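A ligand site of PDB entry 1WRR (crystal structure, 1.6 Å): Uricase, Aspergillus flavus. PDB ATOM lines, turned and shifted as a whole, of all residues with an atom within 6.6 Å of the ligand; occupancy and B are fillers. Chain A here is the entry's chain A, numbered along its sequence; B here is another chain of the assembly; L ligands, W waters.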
ATOM      1  N   SER A 157     -17.172 -14.963 -26.007  1.00  0.00           N
ATOM      2  CA  SER A 157     -16.012 -14.899 -25.114  1.00  0.00           C
ATOM      3  C   SER A 157     -15.032 -15.923 -25.664  1.00  0.00           C
ATOM      4  O   SER A 157     -15.422 -17.030 -26.051  1.00  0.00           O
ATOM      5  CB  SER A 157     -16.393 -15.225 -23.660  1.00  0.00           C
ATOM      6  OG  SER A 157     -15.248 -15.439 -22.858  1.00  0.00           O
ATOM      7  N   GLN A 158     -13.756 -15.540 -25.731  1.00  0.00           N
ATOM      8  CA  GLN A 158     -12.694 -16.377 -26.261  1.00  0.00           C
ATOM      9  C   GLN A 158     -11.550 -16.390 -25.270  1.00  0.00           C
ATOM     10  O   GLN A 158     -11.410 -15.489 -24.431  1.00  0.00           O
ATOM     11  CB  GLN A 158     -12.179 -15.803 -27.601  1.00  0.00           C
ATOM     12  CG  GLN A 158     -13.300 -15.533 -28.592  1.00  0.00           C
ATOM     13  CD  GLN A 158     -12.796 -15.042 -29.941  1.00  0.00           C
ATOM     14  OE1 GLN A 158     -11.630 -15.208 -30.285  1.00  0.00           O
ATOM     15  NE2 GLN A 158     -13.673 -14.424 -30.710  1.00  0.00           N
ATOM     16  N   PHE A 159     -10.709 -17.410 -25.379  1.00  0.00           N
ATOM     17  CA  PHE A 159      -9.456 -17.398 -24.631  1.00  0.00           C
ATOM     18  C   PHE A 159      -8.419 -18.301 -25.291  1.00  0.00           C
ATOM     19  O   PHE A 159      -8.434 -19.522 -25.114  1.00  0.00           O
ATOM     20  CB  PHE A 159      -9.661 -17.744 -23.131  1.00  0.00           C
ATOM     21  CG  PHE A 159      -8.451 -17.446 -22.289  1.00  0.00           C
ATOM     22  CD1 PHE A 159      -7.959 -16.134 -22.167  1.00  0.00           C
ATOM     23  CD2 PHE A 159      -7.770 -18.471 -21.621  1.00  0.00           C
ATOM     24  CE1 PHE A 159      -6.814 -15.862 -21.397  1.00  0.00           C
ATOM     25  CE2 PHE A 159      -6.631 -18.204 -20.835  1.00  0.00           C
ATOM     26  CZ  PHE A 159      -6.141 -16.894 -20.743  1.00  0.00           C
ATOM     27  N   PHE A 162      -2.498 -17.905 -24.865  1.00  0.00           N
ATOM     28  CA  PHE A 162      -1.792 -17.794 -23.604  1.00  0.00           C
ATOM     29  C   PHE A 162      -0.546 -18.673 -23.583  1.00  0.00           C
ATOM     30  O   PHE A 162      -0.371 -19.562 -24.422  1.00  0.00           O
ATOM     31  CB  PHE A 162      -2.713 -18.180 -22.425  1.00  0.00           C
ATOM     32  CG  PHE A 162      -3.467 -19.469 -22.629  1.00  0.00           C
ATOM     33  CD1 PHE A 162      -4.698 -19.464 -23.281  1.00  0.00           C
ATOM     34  CD2 PHE A 162      -2.930 -20.677 -22.163  1.00  0.00           C
ATOM     35  CE1 PHE A 162      -5.407 -20.679 -23.464  1.00  0.00           C
ATOM     36  CE2 PHE A 162      -3.627 -21.873 -22.340  1.00  0.00           C
ATOM     37  CZ  PHE A 162      -4.845 -21.885 -22.999  1.00  0.00           C
ATOM     38  N   LEU A 170      -4.846 -26.674 -20.271  1.00  0.00           N
ATOM     39  CA  LEU A 170      -6.019 -25.981 -20.791  1.00  0.00           C
ATOM     40  C   LEU A 170      -5.985 -25.857 -22.318  1.00  0.00           C
ATOM     41  O   LEU A 170      -4.993 -25.396 -22.867  1.00  0.00           O
ATOM     42  CB  LEU A 170      -6.087 -24.572 -20.177  1.00  0.00           C
ATOM     43  CG  LEU A 170      -7.323 -23.721 -20.566  1.00  0.00           C
ATOM     44  CD1 LEU A 170      -8.627 -24.292 -20.020  1.00  0.00           C
ATOM     45  CD2 LEU A 170      -7.136 -22.277 -20.091  1.00  0.00           C
ATOM     46  N   ARG A 176     -16.684 -19.628 -25.524  1.00  0.00           N
ATOM     47  CA  ARG A 176     -16.926 -20.169 -24.168  1.00  0.00           C
ATOM     48  C   ARG A 176     -17.970 -19.300 -23.471  1.00  0.00           C
ATOM     49  O   ARG A 176     -18.298 -18.185 -23.911  1.00  0.00           O
ATOM     50  CB  ARG A 176     -15.631 -20.214 -23.349  1.00  0.00           C
ATOM     51  CG  ARG A 176     -15.095 -18.830 -22.993  1.00  0.00           C
ATOM     52  CD  ARG A 176     -13.801 -18.883 -22.237  1.00  0.00           C
ATOM     53  NE  ARG A 176     -13.413 -17.530 -21.799  1.00  0.00           N
ATOM     54  CZ  ARG A 176     -12.434 -17.248 -20.933  1.00  0.00           C
ATOM     55  NH1 ARG A 176     -11.723 -18.212 -20.370  1.00  0.00           N
ATOM     56  NH2 ARG A 176     -12.174 -15.963 -20.640  1.00  0.00           N
ATOM     57  N   LEU A 178     -18.947 -16.933 -20.328  1.00  0.00           N
ATOM     58  CA  LEU A 178     -18.235 -16.065 -19.390  1.00  0.00           C
ATOM     59  C   LEU A 178     -19.244 -15.589 -18.348  1.00  0.00           C
ATOM     60  O   LEU A 178     -20.274 -14.998 -18.688  1.00  0.00           O
ATOM     61  CB  LEU A 178     -17.600 -14.881 -20.130  1.00  0.00           C
ATOM     62  CG  LEU A 178     -16.832 -13.884 -19.252  1.00  0.00           C
ATOM     63  CD1 LEU A 178     -15.742 -14.565 -18.436  1.00  0.00           C
ATOM     64  CD2 LEU A 178     -16.230 -12.718 -20.081  1.00  0.00           C
ATOM     65  N   SER A 224     -15.053 -10.800 -26.158  1.00  0.00           N
ATOM     66  CA  SER A 224     -14.003 -10.762 -25.164  1.00  0.00           C
ATOM     67  C   SER A 224     -12.805 -11.643 -25.481  1.00  0.00           C
ATOM     68  O   SER A 224     -12.925 -12.850 -25.688  1.00  0.00           O
ATOM     69  CB  SER A 224     -14.597 -11.126 -23.787  1.00  0.00           C
ATOM     70  OG  SER A 224     -13.576 -11.213 -22.820  1.00  0.00           O
ATOM     71  N   ALA A 225     -11.627 -11.022 -25.489  1.00  0.00           N
ATOM     72  CA  ALA A 225     -10.376 -11.731 -25.690  1.00  0.00           C
ATOM     73  C   ALA A 225      -9.859 -12.381 -24.407  1.00  0.00           C
ATOM     74  O   ALA A 225      -9.025 -13.288 -24.443  1.00  0.00           O
ATOM     75  CB  ALA A 225      -9.328 -10.775 -26.275  1.00  0.00           C
ATOM     76  N   SER A 226     -10.338 -11.871 -23.259  1.00  0.00           N
ATOM     77  CA  SER A 226      -9.938 -12.360 -21.933  1.00  0.00           C
ATOM     78  C   SER A 226     -10.694 -11.501 -20.935  1.00  0.00           C
ATOM     79  O   SER A 226     -11.221 -10.450 -21.295  1.00  0.00           O
ATOM     80  CB  SER A 226      -8.440 -12.217 -21.662  1.00  0.00           C
ATOM     81  OG  SER A 226      -8.058 -10.831 -21.637  1.00  0.00           O
ATOM     82  N   VAL A 227     -10.736 -11.933 -19.668  1.00  0.00           N
ATOM     83  CA  VAL A 227     -11.384 -11.095 -18.662  1.00  0.00           C
ATOM     84  C   VAL A 227     -10.566  -9.799 -18.540  1.00  0.00           C
ATOM     85  O   VAL A 227     -11.157  -8.719 -18.421  1.00  0.00           O
ATOM     86  CB  VAL A 227     -11.511 -11.853 -17.302  1.00  0.00           C
ATOM     87  CG1 VAL A 227     -12.095 -10.944 -16.246  1.00  0.00           C
ATOM     88  CG2 VAL A 227     -12.442 -13.068 -17.499  1.00  0.00           C
ATOM     89  N   GLN A 228      -9.232  -9.937 -18.555  1.00  0.00           N
ATOM     90  CA  GLN A 228      -8.308  -8.791 -18.475  1.00  0.00           C
ATOM     91  C   GLN A 228      -8.678  -7.702 -19.500  1.00  0.00           C
ATOM     92  O   GLN A 228      -8.787  -6.500 -19.164  1.00  0.00           O
ATOM     93  CB  GLN A 228      -6.873  -9.276 -18.756  1.00  0.00           C
ATOM     94  CG  GLN A 228      -6.203 -10.083 -17.609  1.00  0.00           C
ATOM     95  CD  GLN A 228      -6.493 -11.577 -17.606  1.00  0.00           C
ATOM     96  OE1 GLN A 228      -7.499 -12.037 -18.156  1.00  0.00           O
ATOM     97  NE2 GLN A 228      -5.607 -12.332 -16.958  1.00  0.00           N
ATOM     98  N   ASN A 254     -13.728 -15.440 -12.413  1.00  0.00           N
ATOM     99  CA  ASN A 254     -14.141 -16.106 -13.630  1.00  0.00           C
ATOM    100  C   ASN A 254     -14.822 -17.392 -13.130  1.00  0.00           C
ATOM    101  O   ASN A 254     -14.141 -18.280 -12.632  1.00  0.00           O
ATOM    102  CB  ASN A 254     -12.897 -16.372 -14.499  1.00  0.00           C
ATOM    103  CG  ASN A 254     -13.243 -16.919 -15.874  1.00  0.00           C
ATOM    104  OD1 ASN A 254     -14.406 -17.115 -16.222  1.00  0.00           O
ATOM    105  ND2 ASN A 254     -12.214 -17.169 -16.681  1.00  0.00           N
ATOM    106  N   HIS A 256     -16.407 -20.693 -13.625  1.00  0.00           N
ATOM    107  CA  HIS A 256     -16.304 -21.631 -14.776  1.00  0.00           C
ATOM    108  C   HIS A 256     -17.526 -22.509 -14.978  1.00  0.00           C
ATOM    109  O   HIS A 256     -18.100 -23.011 -14.000  1.00  0.00           O
ATOM    110  CB  HIS A 256     -15.073 -22.505 -14.612  1.00  0.00           C
ATOM    111  CG  HIS A 256     -13.813 -21.734 -14.400  1.00  0.00           C
ATOM    112  ND1 HIS A 256     -13.304 -20.863 -15.336  1.00  0.00           N
ATOM    113  CD2 HIS A 256     -12.974 -21.668 -13.337  1.00  0.00           C
ATOM    114  CE1 HIS A 256     -12.183 -20.317 -14.862  1.00  0.00           C
ATOM    115  NE2 HIS A 256     -11.967 -20.783 -13.646  1.00  0.00           N
ATOM    116  N   GLY A 286     -11.136 -18.456 -11.293  1.00  0.00           N
ATOM    117  CA  GLY A 286     -10.116 -17.432 -11.610  1.00  0.00           C
ATOM    118  C   GLY A 286     -10.486 -16.145 -10.871  1.00  0.00           C
ATOM    119  O   GLY A 286     -11.646 -15.920 -10.502  1.00  0.00           O
ATOM    120  N   ILE A 288      -9.395 -11.994 -11.245  1.00  0.00           N
ATOM    121  CA  ILE A 288      -8.639 -11.049 -12.088  1.00  0.00           C
ATOM    122  C   ILE A 288      -8.880  -9.646 -11.555  1.00  0.00           C
ATOM    123  O   ILE A 288     -10.036  -9.260 -11.372  1.00  0.00           O
ATOM    124  CB  ILE A 288      -9.147 -11.097 -13.556  1.00  0.00           C
ATOM    125  CG1 ILE A 288      -9.375 -12.557 -14.056  1.00  0.00           C
ATOM    126  CG2 ILE A 288      -8.153 -10.322 -14.462  1.00  0.00           C
ATOM    127  CD1 ILE A 288      -8.189 -13.412 -14.047  1.00  0.00           C
ATOM    128  N   TYR B   8      -3.541 -11.241 -10.869  1.00  0.00           N
ATOM    129  CA  TYR B   8      -4.566 -12.185 -11.315  1.00  0.00           C
ATOM    130  C   TYR B   8      -4.108 -13.586 -10.890  1.00  0.00           C
ATOM    131  O   TYR B   8      -2.918 -13.834 -10.671  1.00  0.00           O
ATOM    132  CB  TYR B   8      -4.799 -12.099 -12.837  1.00  0.00           C
ATOM    133  CG  TYR B   8      -3.766 -12.868 -13.595  1.00  0.00           C
ATOM    134  CD1 TYR B   8      -2.439 -12.434 -13.647  1.00  0.00           C
ATOM    135  CD2 TYR B   8      -4.071 -14.116 -14.143  1.00  0.00           C
ATOM    136  CE1 TYR B   8      -1.450 -13.212 -14.281  1.00  0.00           C
ATOM    137  CE2 TYR B   8      -3.115 -14.884 -14.776  1.00  0.00           C
ATOM    138  CZ  TYR B   8      -1.798 -14.423 -14.828  1.00  0.00           C
ATOM    139  OH  TYR B   8      -0.829 -15.190 -15.441  1.00  0.00           O
ATOM    140  N   GLY B   9      -5.050 -14.527 -10.781  1.00  0.00           N
ATOM    141  CA  GLY B   9      -4.653 -15.877 -10.419  1.00  0.00           C
ATOM    142  C   GLY B   9      -5.853 -16.766 -10.132  1.00  0.00           C
ATOM    143  O   GLY B   9      -6.887 -16.617 -10.747  1.00  0.00           O
ATOM    144  N   LYS B  10      -5.680 -17.725  -9.215  1.00  0.00           N
ATOM    145  CA  LYS B  10      -6.757 -18.703  -8.953  1.00  0.00           C
ATOM    146  C   LYS B  10      -7.097 -18.620  -7.474  1.00  0.00           C
ATOM    147  O   LYS B  10      -6.194 -18.566  -6.634  1.00  0.00           O
ATOM    148  CB  LYS B  10      -6.283 -20.126  -9.280  1.00  0.00           C
ATOM    149  CG  LYS B  10      -7.419 -21.125  -9.603  1.00  0.00           C
ATOM    150  CD  LYS B  10      -8.090 -20.749 -10.919  1.00  0.00           C
ATOM    151  CE  LYS B  10      -8.743 -21.898 -11.648  1.00  0.00           C
ATOM    152  NZ  LYS B  10      -9.182 -21.450 -13.033  1.00  0.00           N
ATOM    153  N   ASN B  51      -2.419 -12.115 -24.988  1.00  0.00           N
ATOM    154  CA  ASN B  51      -2.425 -13.213 -24.016  1.00  0.00           C
ATOM    155  C   ASN B  51      -1.077 -13.944 -23.847  1.00  0.00           C
ATOM    156  O   ASN B  51      -0.946 -14.810 -22.974  1.00  0.00           O
ATOM    157  CB  ASN B  51      -3.575 -14.204 -24.296  1.00  0.00           C
ATOM    158  CG  ASN B  51      -4.953 -13.590 -24.060  1.00  0.00           C
ATOM    159  OD1 ASN B  51      -5.092 -12.626 -23.291  1.00  0.00           O
ATOM    160  ND2 ASN B  51      -5.968 -14.131 -24.719  1.00  0.00           N
ATOM    161  N   ILE B  54       0.307 -14.178 -20.370  1.00  0.00           N
ATOM    162  CA  ILE B  54      -0.559 -14.793 -19.339  1.00  0.00           C
ATOM    163  C   ILE B  54      -0.245 -16.275 -19.071  1.00  0.00           C
ATOM    164  O   ILE B  54      -0.326 -17.100 -19.981  1.00  0.00           O
ATOM    165  CB  ILE B  54      -2.056 -14.660 -19.681  1.00  0.00           C
ATOM    166  CG1 ILE B  54      -2.481 -13.187 -19.722  1.00  0.00           C
ATOM    167  CG2 ILE B  54      -2.934 -15.413 -18.614  1.00  0.00           C
ATOM    168  CD1 ILE B  54      -3.917 -12.976 -20.221  1.00  0.00           C
ATOM    169  N   VAL B  55       0.113 -16.579 -17.823  1.00  0.00           N
ATOM    170  CA  VAL B  55       0.151 -17.950 -17.322  1.00  0.00           C
ATOM    171  C   VAL B  55      -1.330 -18.208 -16.993  1.00  0.00           C
ATOM    172  O   VAL B  55      -1.875 -17.514 -16.135  1.00  0.00           O
ATOM    173  CB  VAL B  55       1.049 -18.039 -16.056  1.00  0.00           C
ATOM    174  CG1 VAL B  55       0.940 -19.412 -15.369  1.00  0.00           C
ATOM    175  CG2 VAL B  55       2.525 -17.729 -16.402  1.00  0.00           C
ATOM    176  N   ALA B  56      -1.978 -19.125 -17.713  1.00  0.00           N
ATOM    177  CA  ALA B  56      -3.432 -19.324 -17.531  1.00  0.00           C
ATOM    178  C   ALA B  56      -3.757 -19.669 -16.059  1.00  0.00           C
ATOM    179  O   ALA B  56      -2.989 -20.375 -15.406  1.00  0.00           O
ATOM    180  CB  ALA B  56      -3.990 -20.413 -18.496  1.00  0.00           C
ATOM    181  N   THR B  57      -4.894 -19.186 -15.548  1.00  0.00           N
ATOM    182  CA  THR B  57      -5.220 -19.477 -14.150  1.00  0.00           C
ATOM    183  C   THR B  57      -5.377 -20.980 -13.950  1.00  0.00           C
ATOM    184  O   THR B  57      -5.018 -21.484 -12.890  1.00  0.00           O
ATOM    185  CB  THR B  57      -6.446 -18.711 -13.641  1.00  0.00           C
ATOM    186  OG1 THR B  57      -7.607 -19.189 -14.322  1.00  0.00           O
ATOM    187  CG2 THR B  57      -6.286 -17.186 -13.886  1.00  0.00           C
ATOM    188  N   ASP B  58      -5.860 -21.696 -14.982  1.00  0.00           N
ATOM    189  CA  ASP B  58      -5.917 -23.163 -14.910  1.00  0.00           C
ATOM    190  C   ASP B  58      -4.549 -23.796 -14.641  1.00  0.00           C
ATOM    191  O   ASP B  58      -4.414 -24.759 -13.869  1.00  0.00           O
ATOM    192  CB  ASP B  58      -6.518 -23.737 -16.197  1.00  0.00           C
ATOM    193  CG  ASP B  58      -6.838 -25.210 -16.073  1.00  0.00           C
ATOM    194  OD1 ASP B  58      -7.856 -25.546 -15.415  1.00  0.00           O
ATOM    195  OD2 ASP B  58      -6.056 -26.039 -16.600  1.00  0.00           O
ATOM    196  N   SER B  59      -3.495 -23.247 -15.269  1.00  0.00           N
ATOM    197  CA  SER B  59      -2.124 -23.713 -15.036  1.00  0.00           C
ATOM    198  C   SER B  59      -1.630 -23.419 -13.622  1.00  0.00           C
ATOM    199  O   SER B  59      -0.846 -24.186 -13.052  1.00  0.00           O
ATOM    200  CB  SER B  59      -1.165 -23.103 -16.080  1.00  0.00           C
ATOM    201  OG  SER B  59      -1.689 -23.312 -17.369  1.00  0.00           O
HETATM  202  O1  LIG L   1      -9.740 -19.588 -18.385  1.00  0.00           O
HETATM  203  N1  LIG L   1      -8.686 -19.097 -17.989  1.00  0.00           N
HETATM  204  O2  LIG L   1      -7.798 -19.768 -17.409  1.00  0.00           O
HETATM  205  C1  LIG L   1      -8.539 -17.711 -18.097  1.00  0.00           C
HETATM  206  N2  LIG L   1      -9.437 -16.883 -18.656  1.00  0.00           N
HETATM  207  C2  LIG L   1      -9.146 -15.517 -18.667  1.00  0.00           C
HETATM  208  O3  LIG L   1      -9.933 -14.726 -19.202  1.00  0.00           O
HETATM  209  C3  LIG L   1      -7.324 -17.198 -17.500  1.00  0.00           C
HETATM  210  N3  LIG L   1      -6.457 -18.006 -16.947  1.00  0.00           N
HETATM  211  C4  LIG L   1      -7.082 -15.762 -17.539  1.00  0.00           C
HETATM  212  O4  LIG L   1      -6.050 -15.335 -17.004  1.00  0.00           O
HETATM  213  N4  LIG L   1      -8.010 -14.995 -18.121  1.00  0.00           N
HETATM  214  O   HOH W   1      -9.644 -17.374 -15.013  1.00  0.00           O
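Water W1 bridges the side-chain hydroxyl of Thr 57 of chain B (2.8 Å) and the side-chain amide nitrogen of Asn 254 (3.1 Å).
Merely in contact with the ligand: Ala 56 of chain B (3.3 Å), Phe 159 (3.4 Å), Ile 54 of chain B (3.5 Å), Ser 226 (3.6 Å), Asp 58 of chain B (3.7 Å), Tyr 8 of chain B (3.7 Å) and Leu 170 (3.7 Å).
Hydrophobic or aromatic side chains within 4 Å of the ligand: Phe 159, Leu 170, Val 227, Tyr 8 of chain B, Ile 54 of chain B and Ala 56 of chain B.
Of the 26 residues printed, 12 come within 4 Å of the ligand.
Along chain A the residues within 4 Å of the ligand span positions 159 to 254.
The backbone NH (N) of Thr 57 of chain B lies within hydrogen-bond range of an oxygen (O2) of the ligand, at 3.5 Å.
N3 of the ligand lies within hydrogen-bond range of OG1 of Thr 57 of chain B, at 3.1 Å.
NH2 of Arg 176 is in hydrogen-bond range of O3 of the ligand (2.9 Å).
The backbone NH (N) of Val 227 lies within hydrogen-bond range of an oxygen (O3) of the ligand.
The side-chain amide oxygen of Gln 228 is in hydrogen-bond range of a nitrogen (N4) of the ligand.
ND2 of Asn 254 sits close to N2 of the ligand (3.4 Å).
The side-chain amino group (NZ) of Lys 10 of chain B lies within hydrogen-bond range of the side-chain hydroxyl (OG1) of Thr 57 of chain B, at 3.0 Å.
N of Arg 176 sits at hydrogen-bond distance from O of Ser 157, at 2.9 Å.
N of Gln 228 lies close to OG of Ser 226 (3.4 Å).
A ring nitrogen (NE2) of His 256 is in hydrogen-bond range of the backbone carbonyl oxygen (O) of Asn 254.
O of Gly 286 lies within hydrogen-bond range of N of Asn 254, 2.9 Å away.
The backbone carbonyl oxygen of Ser 226 sits at hydrogen-bond distance from the side-chain hydroxyl of Ser 224 (2.9 Å).
OH of Tyr 8 of chain B lies within hydrogen-bond range of O of Val 55 of chain B (2.6 Å).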
